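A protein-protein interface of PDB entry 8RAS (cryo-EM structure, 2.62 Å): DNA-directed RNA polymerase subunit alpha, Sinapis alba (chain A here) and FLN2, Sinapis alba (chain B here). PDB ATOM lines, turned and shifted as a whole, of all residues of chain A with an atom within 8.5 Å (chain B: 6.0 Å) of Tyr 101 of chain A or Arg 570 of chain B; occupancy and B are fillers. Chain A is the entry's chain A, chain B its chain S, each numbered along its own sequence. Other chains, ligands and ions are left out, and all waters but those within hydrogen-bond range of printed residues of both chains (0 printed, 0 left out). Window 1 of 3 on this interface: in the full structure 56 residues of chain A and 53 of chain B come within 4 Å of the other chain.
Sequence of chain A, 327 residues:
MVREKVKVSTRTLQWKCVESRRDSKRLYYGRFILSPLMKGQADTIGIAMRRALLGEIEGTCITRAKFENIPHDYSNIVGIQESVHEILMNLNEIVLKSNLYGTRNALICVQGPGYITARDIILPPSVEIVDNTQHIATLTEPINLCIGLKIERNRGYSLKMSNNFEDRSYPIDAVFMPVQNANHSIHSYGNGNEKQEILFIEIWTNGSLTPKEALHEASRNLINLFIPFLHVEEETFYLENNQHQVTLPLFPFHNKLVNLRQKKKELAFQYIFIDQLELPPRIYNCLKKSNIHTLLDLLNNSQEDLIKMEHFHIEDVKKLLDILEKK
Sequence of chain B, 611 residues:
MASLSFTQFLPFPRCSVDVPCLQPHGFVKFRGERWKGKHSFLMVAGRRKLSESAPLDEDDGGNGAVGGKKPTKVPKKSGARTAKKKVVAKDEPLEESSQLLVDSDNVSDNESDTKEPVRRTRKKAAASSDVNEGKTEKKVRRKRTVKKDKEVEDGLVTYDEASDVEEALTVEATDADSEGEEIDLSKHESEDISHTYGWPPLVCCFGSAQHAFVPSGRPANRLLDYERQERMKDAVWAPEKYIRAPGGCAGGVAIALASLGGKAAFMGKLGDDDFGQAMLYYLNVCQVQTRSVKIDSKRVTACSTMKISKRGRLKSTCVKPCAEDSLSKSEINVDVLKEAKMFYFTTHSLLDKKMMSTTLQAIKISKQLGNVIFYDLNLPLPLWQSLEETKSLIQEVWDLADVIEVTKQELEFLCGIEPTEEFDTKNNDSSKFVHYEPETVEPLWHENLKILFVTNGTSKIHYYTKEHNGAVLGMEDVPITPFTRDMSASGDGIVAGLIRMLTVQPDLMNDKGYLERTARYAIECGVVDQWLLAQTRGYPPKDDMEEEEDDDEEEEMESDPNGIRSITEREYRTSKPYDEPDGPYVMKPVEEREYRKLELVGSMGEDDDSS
The backbone carbonyl oxygen (O) of Arg 573 of chain B sits at hydrogen-bond distance from the backbone NH (N) of Tyr 101 of chain A.
The guanidinium group (NH1) of Arg 104 of chain A sits close to the side-chain hydroxyl (OG) of Ser 575 of chain B.
N of Ser 575 of chain B lies within hydrogen-bond range of O of Tyr 101 of chain A, at 3.0 Å.
OG1 of Thr 568 of chain B lies close to N of Arg 570 of chain B, at 3.5 Å.
The backbone carbonyl oxygen of Arg 104 of chain A is in hydrogen-bond range of the backbone NH of Ile 151 of chain A, at 2.6 Å.
The backbone carbonyl oxygen of Leu 100 of chain A lies within hydrogen-bond range of the guanidinium group of Arg 104 of chain A, 3.2 Å away.
The backbone carbonyl oxygen (O) of Arg 570 of chain B sits at hydrogen-bond distance from the side-chain hydroxyl (OG1) of Thr 574 of chain B.
OH of Tyr 101 of chain A lies within hydrogen-bond range of OE1 of Glu 58 of chain A, 2.8 Å away.
The side-chain carboxylate of Glu 569 of chain B lies within salt-bridge range of the guanidinium group of Arg 573 of chain B, at 3.6 Å.
Leu 100 of chain A touches Arg 573 of chain B (CA to O, 3.2 Å).
CB of Leu 100 of chain A touches OG of Ser 575 of chain B (3.4 Å).
Tyr 101 of chain A touches Arg 570 of chain B.
O of Tyr 101 of chain A touches CA of Thr 574 of chain B, at 3.6 Å.
CD of Arg 104 of chain A touches O of Lys 576 of chain B, 3.6 Å away.
Of the printed residues of chain B, Leu 100 of chain A touches Arg 573 and Ser 575.
Of the printed residues of chain B, Tyr 101 of chain A touches Arg 570, Arg 573, Thr 574 and Ser 575.
Printed residues of chain B within 4 Å of Arg 104 of chain A: Ser 575 and Lys 576.
Arg 570 of chain B touches just one residue of chain A: Tyr 101 (3.7 Å).
Of the printed residues of chain A, Ser 575 of chain B touches Leu 100, Tyr 101 and Arg 104.
Printed residues of chain A within 4 Å of Lys 576 of chain B: Arg 104.
The nearest residue of chain B that does not touch Tyr 101 of chain A is Glu 569 of chain B (5.4 Å).
Along chain B the printed residues that touch a printed residue of chain A span positions 570 to 576.
Of the 21 printed residues of chain A, 3 touch a printed residue of chain B.
Printed residues of chain A that touch a printed residue of chain B: Leu 100, Tyr 101 and Arg 104.
Hydrophobic or aromatic side chains of chain A within 4 Å of the printed part of chain B: Leu 100 and Tyr 101.
Among the printed residues, 8 pairs touch across the chains.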
ATOM      1  N   GLU A  56     -18.062 -17.735  10.948  1.00  0.00           N
ATOM      2  CA  GLU A  56     -17.881 -17.063   9.668  1.00  0.00           C
ATOM      3  C   GLU A  56     -18.076 -15.553   9.721  1.00  0.00           C
ATOM      4  O   GLU A  56     -17.930 -14.893   8.689  1.00  0.00           O
ATOM      5  CB  GLU A  56     -18.829 -17.661   8.623  1.00  0.00           C
ATOM      6  CG  GLU A  56     -18.535 -19.111   8.280  1.00  0.00           C
ATOM      7  CD  GLU A  56     -17.101 -19.325   7.833  1.00  0.00           C
ATOM      8  OE1 GLU A  56     -16.592 -18.500   7.046  1.00  0.00           O
ATOM      9  OE2 GLU A  56     -16.482 -20.319   8.268  1.00  0.00           O
ATOM     10  N   ILE A  57     -18.391 -14.987  10.881  1.00  0.00           N
ATOM     11  CA  ILE A  57     -18.639 -13.555  11.010  1.00  0.00           C
ATOM     12  C   ILE A  57     -17.385 -12.889  11.559  1.00  0.00           C
ATOM     13  O   ILE A  57     -16.794 -13.366  12.534  1.00  0.00           O
ATOM     14  CB  ILE A  57     -19.861 -13.279  11.901  1.00  0.00           C
ATOM     15  CG1 ILE A  57     -21.121 -13.833  11.235  1.00  0.00           C
ATOM     16  CG2 ILE A  57     -20.015 -11.793  12.157  1.00  0.00           C
ATOM     17  CD1 ILE A  57     -22.384 -13.524  11.974  1.00  0.00           C
ATOM     18  N   GLU A  58     -16.978 -11.792  10.929  1.00  0.00           N
ATOM     19  CA  GLU A  58     -15.719 -11.128  11.227  1.00  0.00           C
ATOM     20  C   GLU A  58     -15.932  -9.909  12.115  1.00  0.00           C
ATOM     21  O   GLU A  58     -16.996  -9.285  12.106  1.00  0.00           O
ATOM     22  CB  GLU A  58     -15.019 -10.706   9.936  1.00  0.00           C
ATOM     23  CG  GLU A  58     -14.620 -11.864   9.050  1.00  0.00           C
ATOM     24  CD  GLU A  58     -13.771 -11.429   7.879  1.00  0.00           C
ATOM     25  OE1 GLU A  58     -14.268 -10.639   7.051  1.00  0.00           O
ATOM     26  OE2 GLU A  58     -12.609 -11.874   7.785  1.00  0.00           O
ATOM     27  N   GLY A  59     -14.895  -9.574  12.888  1.00  0.00           N
ATOM     28  CA  GLY A  59     -14.930  -8.409  13.745  1.00  0.00           C
ATOM     29  C   GLY A  59     -13.607  -7.670  13.710  1.00  0.00           C
ATOM     30  O   GLY A  59     -12.621  -8.144  13.145  1.00  0.00           O
ATOM     31  N   THR A  60     -13.606  -6.490  14.325  1.00  0.00           N
ATOM     32  CA  THR A  60     -12.430  -5.636  14.399  1.00  0.00           C
ATOM     33  C   THR A  60     -12.061  -5.398  15.855  1.00  0.00           C
ATOM     34  O   THR A  60     -12.935  -5.160  16.695  1.00  0.00           O
ATOM     35  CB  THR A  60     -12.670  -4.290  13.708  1.00  0.00           C
ATOM     36  OG1 THR A  60     -13.651  -3.545  14.439  1.00  0.00           O
ATOM     37  CG2 THR A  60     -13.171  -4.504  12.297  1.00  0.00           C
ATOM     38  N   SER A  98     -16.153  -2.007  12.119  1.00  0.00           N
ATOM     39  CA  SER A  98     -15.669  -1.515  10.839  1.00  0.00           C
ATOM     40  C   SER A  98     -16.090  -2.492   9.753  1.00  0.00           C
ATOM     41  O   SER A  98     -16.192  -3.698   9.992  1.00  0.00           O
ATOM     42  CB  SER A  98     -14.148  -1.337  10.835  1.00  0.00           C
ATOM     43  OG  SER A  98     -13.691  -0.883   9.574  1.00  0.00           O
ATOM     44  N   ASN A  99     -16.335  -1.957   8.560  1.00  0.00           N
ATOM     45  CA  ASN A  99     -16.719  -2.756   7.408  1.00  0.00           C
ATOM     46  C   ASN A  99     -15.562  -3.014   6.454  1.00  0.00           C
ATOM     47  O   ASN A  99     -15.765  -3.654   5.418  1.00  0.00           O
ATOM     48  CB  ASN A  99     -17.860  -2.073   6.648  1.00  0.00           C
ATOM     49  CG  ASN A  99     -19.128  -1.969   7.466  1.00  0.00           C
ATOM     50  OD1 ASN A  99     -19.471  -2.878   8.220  1.00  0.00           O
ATOM     51  ND2 ASN A  99     -19.836  -0.857   7.319  1.00  0.00           N
ATOM     52  N   LEU A 100     -14.362  -2.540   6.774  1.00  0.00           N
ATOM     53  CA  LEU A 100     -13.236  -2.587   5.856  1.00  0.00           C
ATOM     54  C   LEU A 100     -12.097  -3.412   6.439  1.00  0.00           C
ATOM     55  O   LEU A 100     -12.027  -3.655   7.646  1.00  0.00           O
ATOM     56  CB  LEU A 100     -12.738  -1.176   5.522  1.00  0.00           C
ATOM     57  CG  LEU A 100     -13.794  -0.210   4.985  1.00  0.00           C
ATOM     58  CD1 LEU A 100     -13.223   1.187   4.850  1.00  0.00           C
ATOM     59  CD2 LEU A 100     -14.339  -0.701   3.655  1.00  0.00           C
ATOM     60  N   TYR A 101     -11.203  -3.841   5.556  1.00  0.00           N
ATOM     61  CA  TYR A 101     -10.046  -4.641   5.920  1.00  0.00           C
ATOM     62  C   TYR A 101      -8.782  -3.790   5.900  1.00  0.00           C
ATOM     63  O   TYR A 101      -8.773  -2.648   5.435  1.00  0.00           O
ATOM     64  CB  TYR A 101      -9.894  -5.834   4.971  1.00  0.00           C
ATOM     65  CG  TYR A 101     -11.111  -6.721   4.895  1.00  0.00           C
ATOM     66  CD1 TYR A 101     -11.286  -7.768   5.789  1.00  0.00           C
ATOM     67  CD2 TYR A 101     -12.085  -6.515   3.930  1.00  0.00           C
ATOM     68  CE1 TYR A 101     -12.396  -8.580   5.724  1.00  0.00           C
ATOM     69  CE2 TYR A 101     -13.199  -7.322   3.857  1.00  0.00           C
ATOM     70  CZ  TYR A 101     -13.350  -8.353   4.757  1.00  0.00           C
ATOM     71  OH  TYR A 101     -14.459  -9.162   4.688  1.00  0.00           O
ATOM     72  N   GLY A 102      -7.705  -4.366   6.407  1.00  0.00           N
ATOM     73  CA  GLY A 102      -6.428  -3.693   6.474  1.00  0.00           C
ATOM     74  C   GLY A 102      -6.056  -3.325   7.902  1.00  0.00           C
ATOM     75  O   GLY A 102      -6.891  -3.279   8.808  1.00  0.00           O
ATOM     76  N   THR A 103      -4.765  -3.050   8.092  1.00  0.00           N
ATOM     77  CA  THR A 103      -4.220  -2.753   9.417  1.00  0.00           C
ATOM     78  C   THR A 103      -4.252  -1.244   9.643  1.00  0.00           C
ATOM     79  O   THR A 103      -3.268  -0.527   9.450  1.00  0.00           O
ATOM     80  CB  THR A 103      -2.812  -3.315   9.556  1.00  0.00           C
ATOM     81  OG1 THR A 103      -2.772  -4.639   9.010  1.00  0.00           O
ATOM     82  CG2 THR A 103      -2.401  -3.365  11.019  1.00  0.00           C
ATOM     83  N   ARG A 104      -5.415  -0.760  10.064  1.00  0.00           N
ATOM     84  CA  ARG A 104      -5.548   0.628  10.472  1.00  0.00           C
ATOM     85  C   ARG A 104      -4.838   0.851  11.803  1.00  0.00           C
ATOM     86  O   ARG A 104      -4.623  -0.077  12.586  1.00  0.00           O
ATOM     87  CB  ARG A 104      -7.020   1.018  10.595  1.00  0.00           C
ATOM     88  CG  ARG A 104      -7.637   1.598   9.333  1.00  0.00           C
ATOM     89  CD  ARG A 104      -7.804   0.545   8.252  1.00  0.00           C
ATOM     90  NE  ARG A 104      -8.205  -0.748   8.795  1.00  0.00           N
ATOM     91  CZ  ARG A 104      -9.460  -1.129   8.983  1.00  0.00           C
ATOM     92  NH1 ARG A 104     -10.475  -0.335   8.687  1.00  0.00           N
ATOM     93  NH2 ARG A 104      -9.703  -2.337   9.481  1.00  0.00           N
ATOM     94  N   SER A 126     -12.892   5.074   9.331  1.00  0.00           N
ATOM     95  CA  SER A 126     -13.535   3.808   9.007  1.00  0.00           C
ATOM     96  C   SER A 126     -13.821   2.941  10.228  1.00  0.00           C
ATOM     97  O   SER A 126     -14.421   1.872  10.078  1.00  0.00           O
ATOM     98  CB  SER A 126     -12.672   3.024   8.014  1.00  0.00           C
ATOM     99  OG  SER A 126     -11.296   3.162   8.315  1.00  0.00           O
ATOM    100  N   VAL A 127     -13.417   3.368  11.422  1.00  0.00           N
ATOM    101  CA  VAL A 127     -13.571   2.584  12.643  1.00  0.00           C
ATOM    102  C   VAL A 127     -14.372   3.395  13.651  1.00  0.00           C
ATOM    103  O   VAL A 127     -14.185   4.610  13.773  1.00  0.00           O
ATOM    104  CB  VAL A 127     -12.204   2.178  13.232  1.00  0.00           C
ATOM    105  CG1 VAL A 127     -12.379   1.139  14.327  1.00  0.00           C
ATOM    106  CG2 VAL A 127     -11.289   1.652  12.142  1.00  0.00           C
ATOM    107  N   ILE A 151      -5.259  -1.776  14.380  1.00  0.00           N
ATOM    108  CA  ILE A 151      -6.598  -2.337  14.249  1.00  0.00           C
ATOM    109  C   ILE A 151      -6.731  -2.964  12.870  1.00  0.00           C
ATOM    110  O   ILE A 151      -6.405  -2.328  11.862  1.00  0.00           O
ATOM    111  CB  ILE A 151      -7.684  -1.264  14.453  1.00  0.00           C
ATOM    112  CG1 ILE A 151      -7.498  -0.561  15.797  1.00  0.00           C
ATOM    113  CG2 ILE A 151      -9.068  -1.879  14.351  1.00  0.00           C
ATOM    114  CD1 ILE A 151      -7.984   0.864  15.806  1.00  0.00           C
ATOM    115  N   GLU A 152      -7.207  -4.207  12.823  1.00  0.00           N
ATOM    116  CA  GLU A 152      -7.548  -4.838  11.557  1.00  0.00           C
ATOM    117  C   GLU A 152      -8.778  -5.712  11.738  1.00  0.00           C
ATOM    118  O   GLU A 152      -9.124  -6.121  12.848  1.00  0.00           O
ATOM    119  CB  GLU A 152      -6.395  -5.674  10.980  1.00  0.00           C
ATOM    120  CG  GLU A 152      -5.966  -6.871  11.810  1.00  0.00           C
ATOM    121  CD  GLU A 152      -5.022  -6.506  12.934  1.00  0.00           C
ATOM    122  OE1 GLU A 152      -5.231  -5.462  13.585  1.00  0.00           O
ATOM    123  OE2 GLU A 152      -4.058  -7.264  13.167  1.00  0.00           O
ATOM    124  N   ARG A 153      -9.439  -5.987  10.618  1.00  0.00           N
ATOM    125  CA  ARG A 153     -10.626  -6.827  10.573  1.00  0.00           C
ATOM    126  C   ARG A 153     -10.218  -8.238  10.178  1.00  0.00           C
ATOM    127  O   ARG A 153      -9.471  -8.424   9.212  1.00  0.00           O
ATOM    128  CB  ARG A 153     -11.642  -6.263   9.580  1.00  0.00           C
ATOM    129  CG  ARG A 153     -12.955  -7.014   9.508  1.00  0.00           C
ATOM    130  CD  ARG A 153     -13.966  -6.227   8.695  1.00  0.00           C
ATOM    131  NE  ARG A 153     -15.012  -7.077   8.144  1.00  0.00           N
ATOM    132  CZ  ARG A 153     -16.261  -7.108   8.584  1.00  0.00           C
ATOM    133  NH1 ARG A 153     -16.660  -6.341   9.585  1.00  0.00           N
ATOM    134  NH2 ARG A 153     -17.133  -7.927   8.005  1.00  0.00           N
ATOM    135  N   ASN A 154     -10.704  -9.226  10.921  1.00  0.00           N
ATOM    136  CA  ASN A 154     -10.299 -10.609  10.710  1.00  0.00           C
ATOM    137  C   ASN A 154     -11.380 -11.526  11.262  1.00  0.00           C
ATOM    138  O   ASN A 154     -12.389 -11.073  11.809  1.00  0.00           O
ATOM    139  CB  ASN A 154      -8.942 -10.886  11.364  1.00  0.00           C
ATOM    140  CG  ASN A 154      -8.051 -11.760  10.511  1.00  0.00           C
ATOM    141  OD1 ASN A 154      -8.508 -12.724   9.897  1.00  0.00           O
ATOM    142  ND2 ASN A 154      -6.765 -11.431  10.469  1.00  0.00           N
ATOM    143  N   ARG A 155     -11.158 -12.828  11.117  1.00  0.00           N
ATOM    144  CA  ARG A 155     -12.051 -13.850  11.637  1.00  0.00           C
ATOM    145  C   ARG A 155     -11.309 -14.708  12.651  1.00  0.00           C
ATOM    146  O   ARG A 155     -10.085 -14.854  12.589  1.00  0.00           O
ATOM    147  CB  ARG A 155     -12.597 -14.738  10.515  1.00  0.00           C
ATOM    148  CG  ARG A 155     -11.534 -15.233   9.551  1.00  0.00           C
ATOM    149  CD  ARG A 155     -12.148 -15.973   8.376  1.00  0.00           C
ATOM    150  NE  ARG A 155     -12.251 -17.404   8.633  1.00  0.00           N
ATOM    151  CZ  ARG A 155     -13.320 -18.137   8.361  1.00  0.00           C
ATOM    152  NH1 ARG A 155     -14.403 -17.605   7.821  1.00  0.00           N
ATOM    153  NH2 ARG A 155     -13.304 -19.437   8.638  1.00  0.00           N
ATOM    154  N   GLU A 217     -25.635 -11.051   7.699  1.00  0.00           N
ATOM    155  CA  GLU A 217     -24.254 -11.326   7.326  1.00  0.00           C
ATOM    156  C   GLU A 217     -23.991 -12.822   7.248  1.00  0.00           C
ATOM    157  O   GLU A 217     -23.266 -13.284   6.363  1.00  0.00           O
ATOM    158  CB  GLU A 217     -23.304 -10.659   8.320  1.00  0.00           C
ATOM    159  CG  GLU A 217     -21.932 -11.301   8.402  1.00  0.00           C
ATOM    160  CD  GLU A 217     -20.811 -10.285   8.412  1.00  0.00           C
ATOM    161  OE1 GLU A 217     -21.106  -9.073   8.453  1.00  0.00           O
ATOM    162  OE2 GLU A 217     -19.634 -10.700   8.376  1.00  0.00           O
ATOM    163  N   ASN A 221     -22.734 -14.717   3.943  1.00  0.00           N
ATOM    164  CA  ASN A 221     -21.511 -15.510   3.980  1.00  0.00           C
ATOM    165  C   ASN A 221     -21.774 -16.949   3.559  1.00  0.00           C
ATOM    166  O   ASN A 221     -20.974 -17.545   2.830  1.00  0.00           O
ATOM    167  CB  ASN A 221     -20.899 -15.462   5.379  1.00  0.00           C
ATOM    168  CG  ASN A 221     -20.255 -14.127   5.686  1.00  0.00           C
ATOM    169  OD1 ASN A 221     -20.088 -13.287   4.805  1.00  0.00           O
ATOM    170  ND2 ASN A 221     -19.890 -13.924   6.945  1.00  0.00           N
ATOM    171  N   THR B 568     -10.878  -7.578  -6.611  1.00  0.00           N
ATOM    172  CA  THR B 568     -11.896  -8.389  -5.966  1.00  0.00           C
ATOM    173  C   THR B 568     -12.696  -7.552  -4.972  1.00  0.00           C
ATOM    174  O   THR B 568     -12.345  -6.415  -4.645  1.00  0.00           O
ATOM    175  CB  THR B 568     -11.264  -9.585  -5.256  1.00  0.00           C
ATOM    176  OG1 THR B 568     -10.397  -9.125  -4.212  1.00  0.00           O
ATOM    177  CG2 THR B 568     -10.468 -10.429  -6.235  1.00  0.00           C
ATOM    178  N   GLU B 569     -13.801  -8.131  -4.498  1.00  0.00           N
ATOM    179  CA  GLU B 569     -14.575  -7.485  -3.447  1.00  0.00           C
ATOM    180  C   GLU B 569     -13.760  -7.345  -2.169  1.00  0.00           C
ATOM    181  O   GLU B 569     -13.950  -6.389  -1.410  1.00  0.00           O
ATOM    182  CB  GLU B 569     -15.856  -8.275  -3.183  1.00  0.00           C
ATOM    183  CG  GLU B 569     -16.841  -7.585  -2.260  1.00  0.00           C
ATOM    184  CD  GLU B 569     -17.841  -8.549  -1.657  1.00  0.00           C
ATOM    185  OE1 GLU B 569     -17.515  -9.184  -0.631  1.00  0.00           O
ATOM    186  OE2 GLU B 569     -18.955  -8.676  -2.207  1.00  0.00           O
ATOM    187  N   ARG B 570     -12.849  -8.287  -1.917  1.00  0.00           N
ATOM    188  CA  ARG B 570     -11.963  -8.181  -0.764  1.00  0.00           C
ATOM    189  C   ARG B 570     -11.031  -6.982  -0.891  1.00  0.00           C
ATOM    190  O   ARG B 570     -10.807  -6.256   0.083  1.00  0.00           O
ATOM    191  CB  ARG B 570     -11.165  -9.474  -0.607  1.00  0.00           C
ATOM    192  CG  ARG B 570     -10.239  -9.501   0.591  1.00  0.00           C
ATOM    193  CD  ARG B 570     -11.026  -9.547   1.884  1.00  0.00           C
ATOM    194  NE  ARG B 570     -10.846 -10.812   2.587  1.00  0.00           N
ATOM    195  CZ  ARG B 570      -9.908 -11.036   3.496  1.00  0.00           C
ATOM    196  NH1 ARG B 570      -9.038 -10.099   3.836  1.00  0.00           N
ATOM    197  NH2 ARG B 570      -9.840 -12.230   4.077  1.00  0.00           N
ATOM    198  N   GLU B 571     -10.472  -6.762  -2.085  1.00  0.00           N
ATOM    199  CA  GLU B 571      -9.608  -5.604  -2.295  1.00  0.00           C
ATOM    200  C   GLU B 571     -10.402  -4.306  -2.309  1.00  0.00           C
ATOM    201  O   GLU B 571      -9.895  -3.268  -1.870  1.00  0.00           O
ATOM    202  CB  GLU B 571      -8.826  -5.755  -3.599  1.00  0.00           C
ATOM    203  CG  GLU B 571      -7.901  -6.956  -3.642  1.00  0.00           C
ATOM    204  CD  GLU B 571      -7.389  -7.240  -5.039  1.00  0.00           C
ATOM    205  OE1 GLU B 571      -6.764  -6.340  -5.638  1.00  0.00           O
ATOM    206  OE2 GLU B 571      -7.609  -8.363  -5.538  1.00  0.00           O
ATOM    207  N   TYR B 572     -11.635  -4.342  -2.817  1.00  0.00           N
ATOM    208  CA  TYR B 572     -12.466  -3.144  -2.832  1.00  0.00           C
ATOM    209  C   TYR B 572     -12.770  -2.667  -1.419  1.00  0.00           C
ATOM    210  O   TYR B 572     -12.787  -1.460  -1.151  1.00  0.00           O
ATOM    211  CB  TYR B 572     -13.761  -3.418  -3.598  1.00  0.00           C
ATOM    212  CG  TYR B 572     -14.659  -2.212  -3.733  1.00  0.00           C
ATOM    213  CD1 TYR B 572     -14.332  -1.172  -4.592  1.00  0.00           C
ATOM    214  CD2 TYR B 572     -15.833  -2.111  -3.000  1.00  0.00           C
ATOM    215  CE1 TYR B 572     -15.147  -0.068  -4.718  1.00  0.00           C
ATOM    216  CE2 TYR B 572     -16.656  -1.009  -3.120  1.00  0.00           C
ATOM    217  CZ  TYR B 572     -16.307   0.009  -3.980  1.00  0.00           C
ATOM    218  OH  TYR B 572     -17.122   1.109  -4.103  1.00  0.00           O
ATOM    219  N   ARG B 573     -13.012  -3.599  -0.499  1.00  0.00           N
ATOM    220  CA  ARG B 573     -13.330  -3.281   0.884  1.00  0.00           C
ATOM    221  C   ARG B 573     -12.092  -3.185   1.767  1.00  0.00           C
ATOM    222  O   ARG B 573     -12.193  -3.386   2.981  1.00  0.00           O
ATOM    223  CB  ARG B 573     -14.300  -4.318   1.452  1.00  0.00           C
ATOM    224  CG  ARG B 573     -15.597  -4.429   0.680  1.00  0.00           C
ATOM    225  CD  ARG B 573     -16.498  -5.502   1.259  1.00  0.00           C
ATOM    226  NE  ARG B 573     -17.757  -5.598   0.531  1.00  0.00           N
ATOM    227  CZ  ARG B 573     -18.849  -6.186   0.997  1.00  0.00           C
ATOM    228  NH1 ARG B 573     -18.874  -6.748   2.194  1.00  0.00           N
ATOM    229  NH2 ARG B 573     -19.944  -6.211   0.243  1.00  0.00           N
ATOM    230  N   THR B 574     -10.932  -2.894   1.189  1.00  0.00           N
ATOM    231  CA  THR B 574      -9.701  -2.700   1.941  1.00  0.00           C
ATOM    232  C   THR B 574      -9.372  -1.216   1.978  1.00  0.00           C
ATOM    233  O   THR B 574      -9.327  -0.560   0.934  1.00  0.00           O
ATOM    234  CB  THR B 574      -8.545  -3.486   1.323  1.00  0.00           C
ATOM    235  OG1 THR B 574      -8.878  -4.879   1.285  1.00  0.00           O
ATOM    236  CG2 THR B 574      -7.279  -3.301   2.142  1.00  0.00           C
ATOM    237  N   SER B 575      -9.142  -0.693   3.177  1.00  0.00           N
ATOM    238  CA  SER B 575      -8.856   0.719   3.373  1.00  0.00           C
ATOM    239  C   SER B 575      -7.354   0.958   3.477  1.00  0.00           C
ATOM    240  O   SER B 575      -6.552   0.031   3.610  1.00  0.00           O
ATOM    241  CB  SER B 575      -9.568   1.238   4.625  1.00  0.00           C
ATOM    242  OG  SER B 575      -9.639   0.231   5.617  1.00  0.00           O
ATOM    243  N   LYS B 576      -6.980   2.233   3.407  1.00  0.00           N
ATOM    244  CA  LYS B 576      -5.587   2.611   3.552  1.00  0.00           C
ATOM    245  C   LYS B 576      -5.144   2.460   5.008  1.00  0.00           C
ATOM    246  O   LYS B 576      -5.961   2.562   5.927  1.00  0.00           O
ATOM    247  CB  LYS B 576      -5.373   4.049   3.086  1.00  0.00           C
ATOM    248  CG  LYS B 576      -6.419   5.028   3.591  1.00  0.00           C
ATOM    249  CD  LYS B 576      -6.012   6.463   3.302  1.00  0.00           C
ATOM    250  CE  LYS B 576      -5.980   6.737   1.808  1.00  0.00           C
ATOM    251  NZ  LYS B 576      -5.771   8.182   1.517  1.00  0.00           N
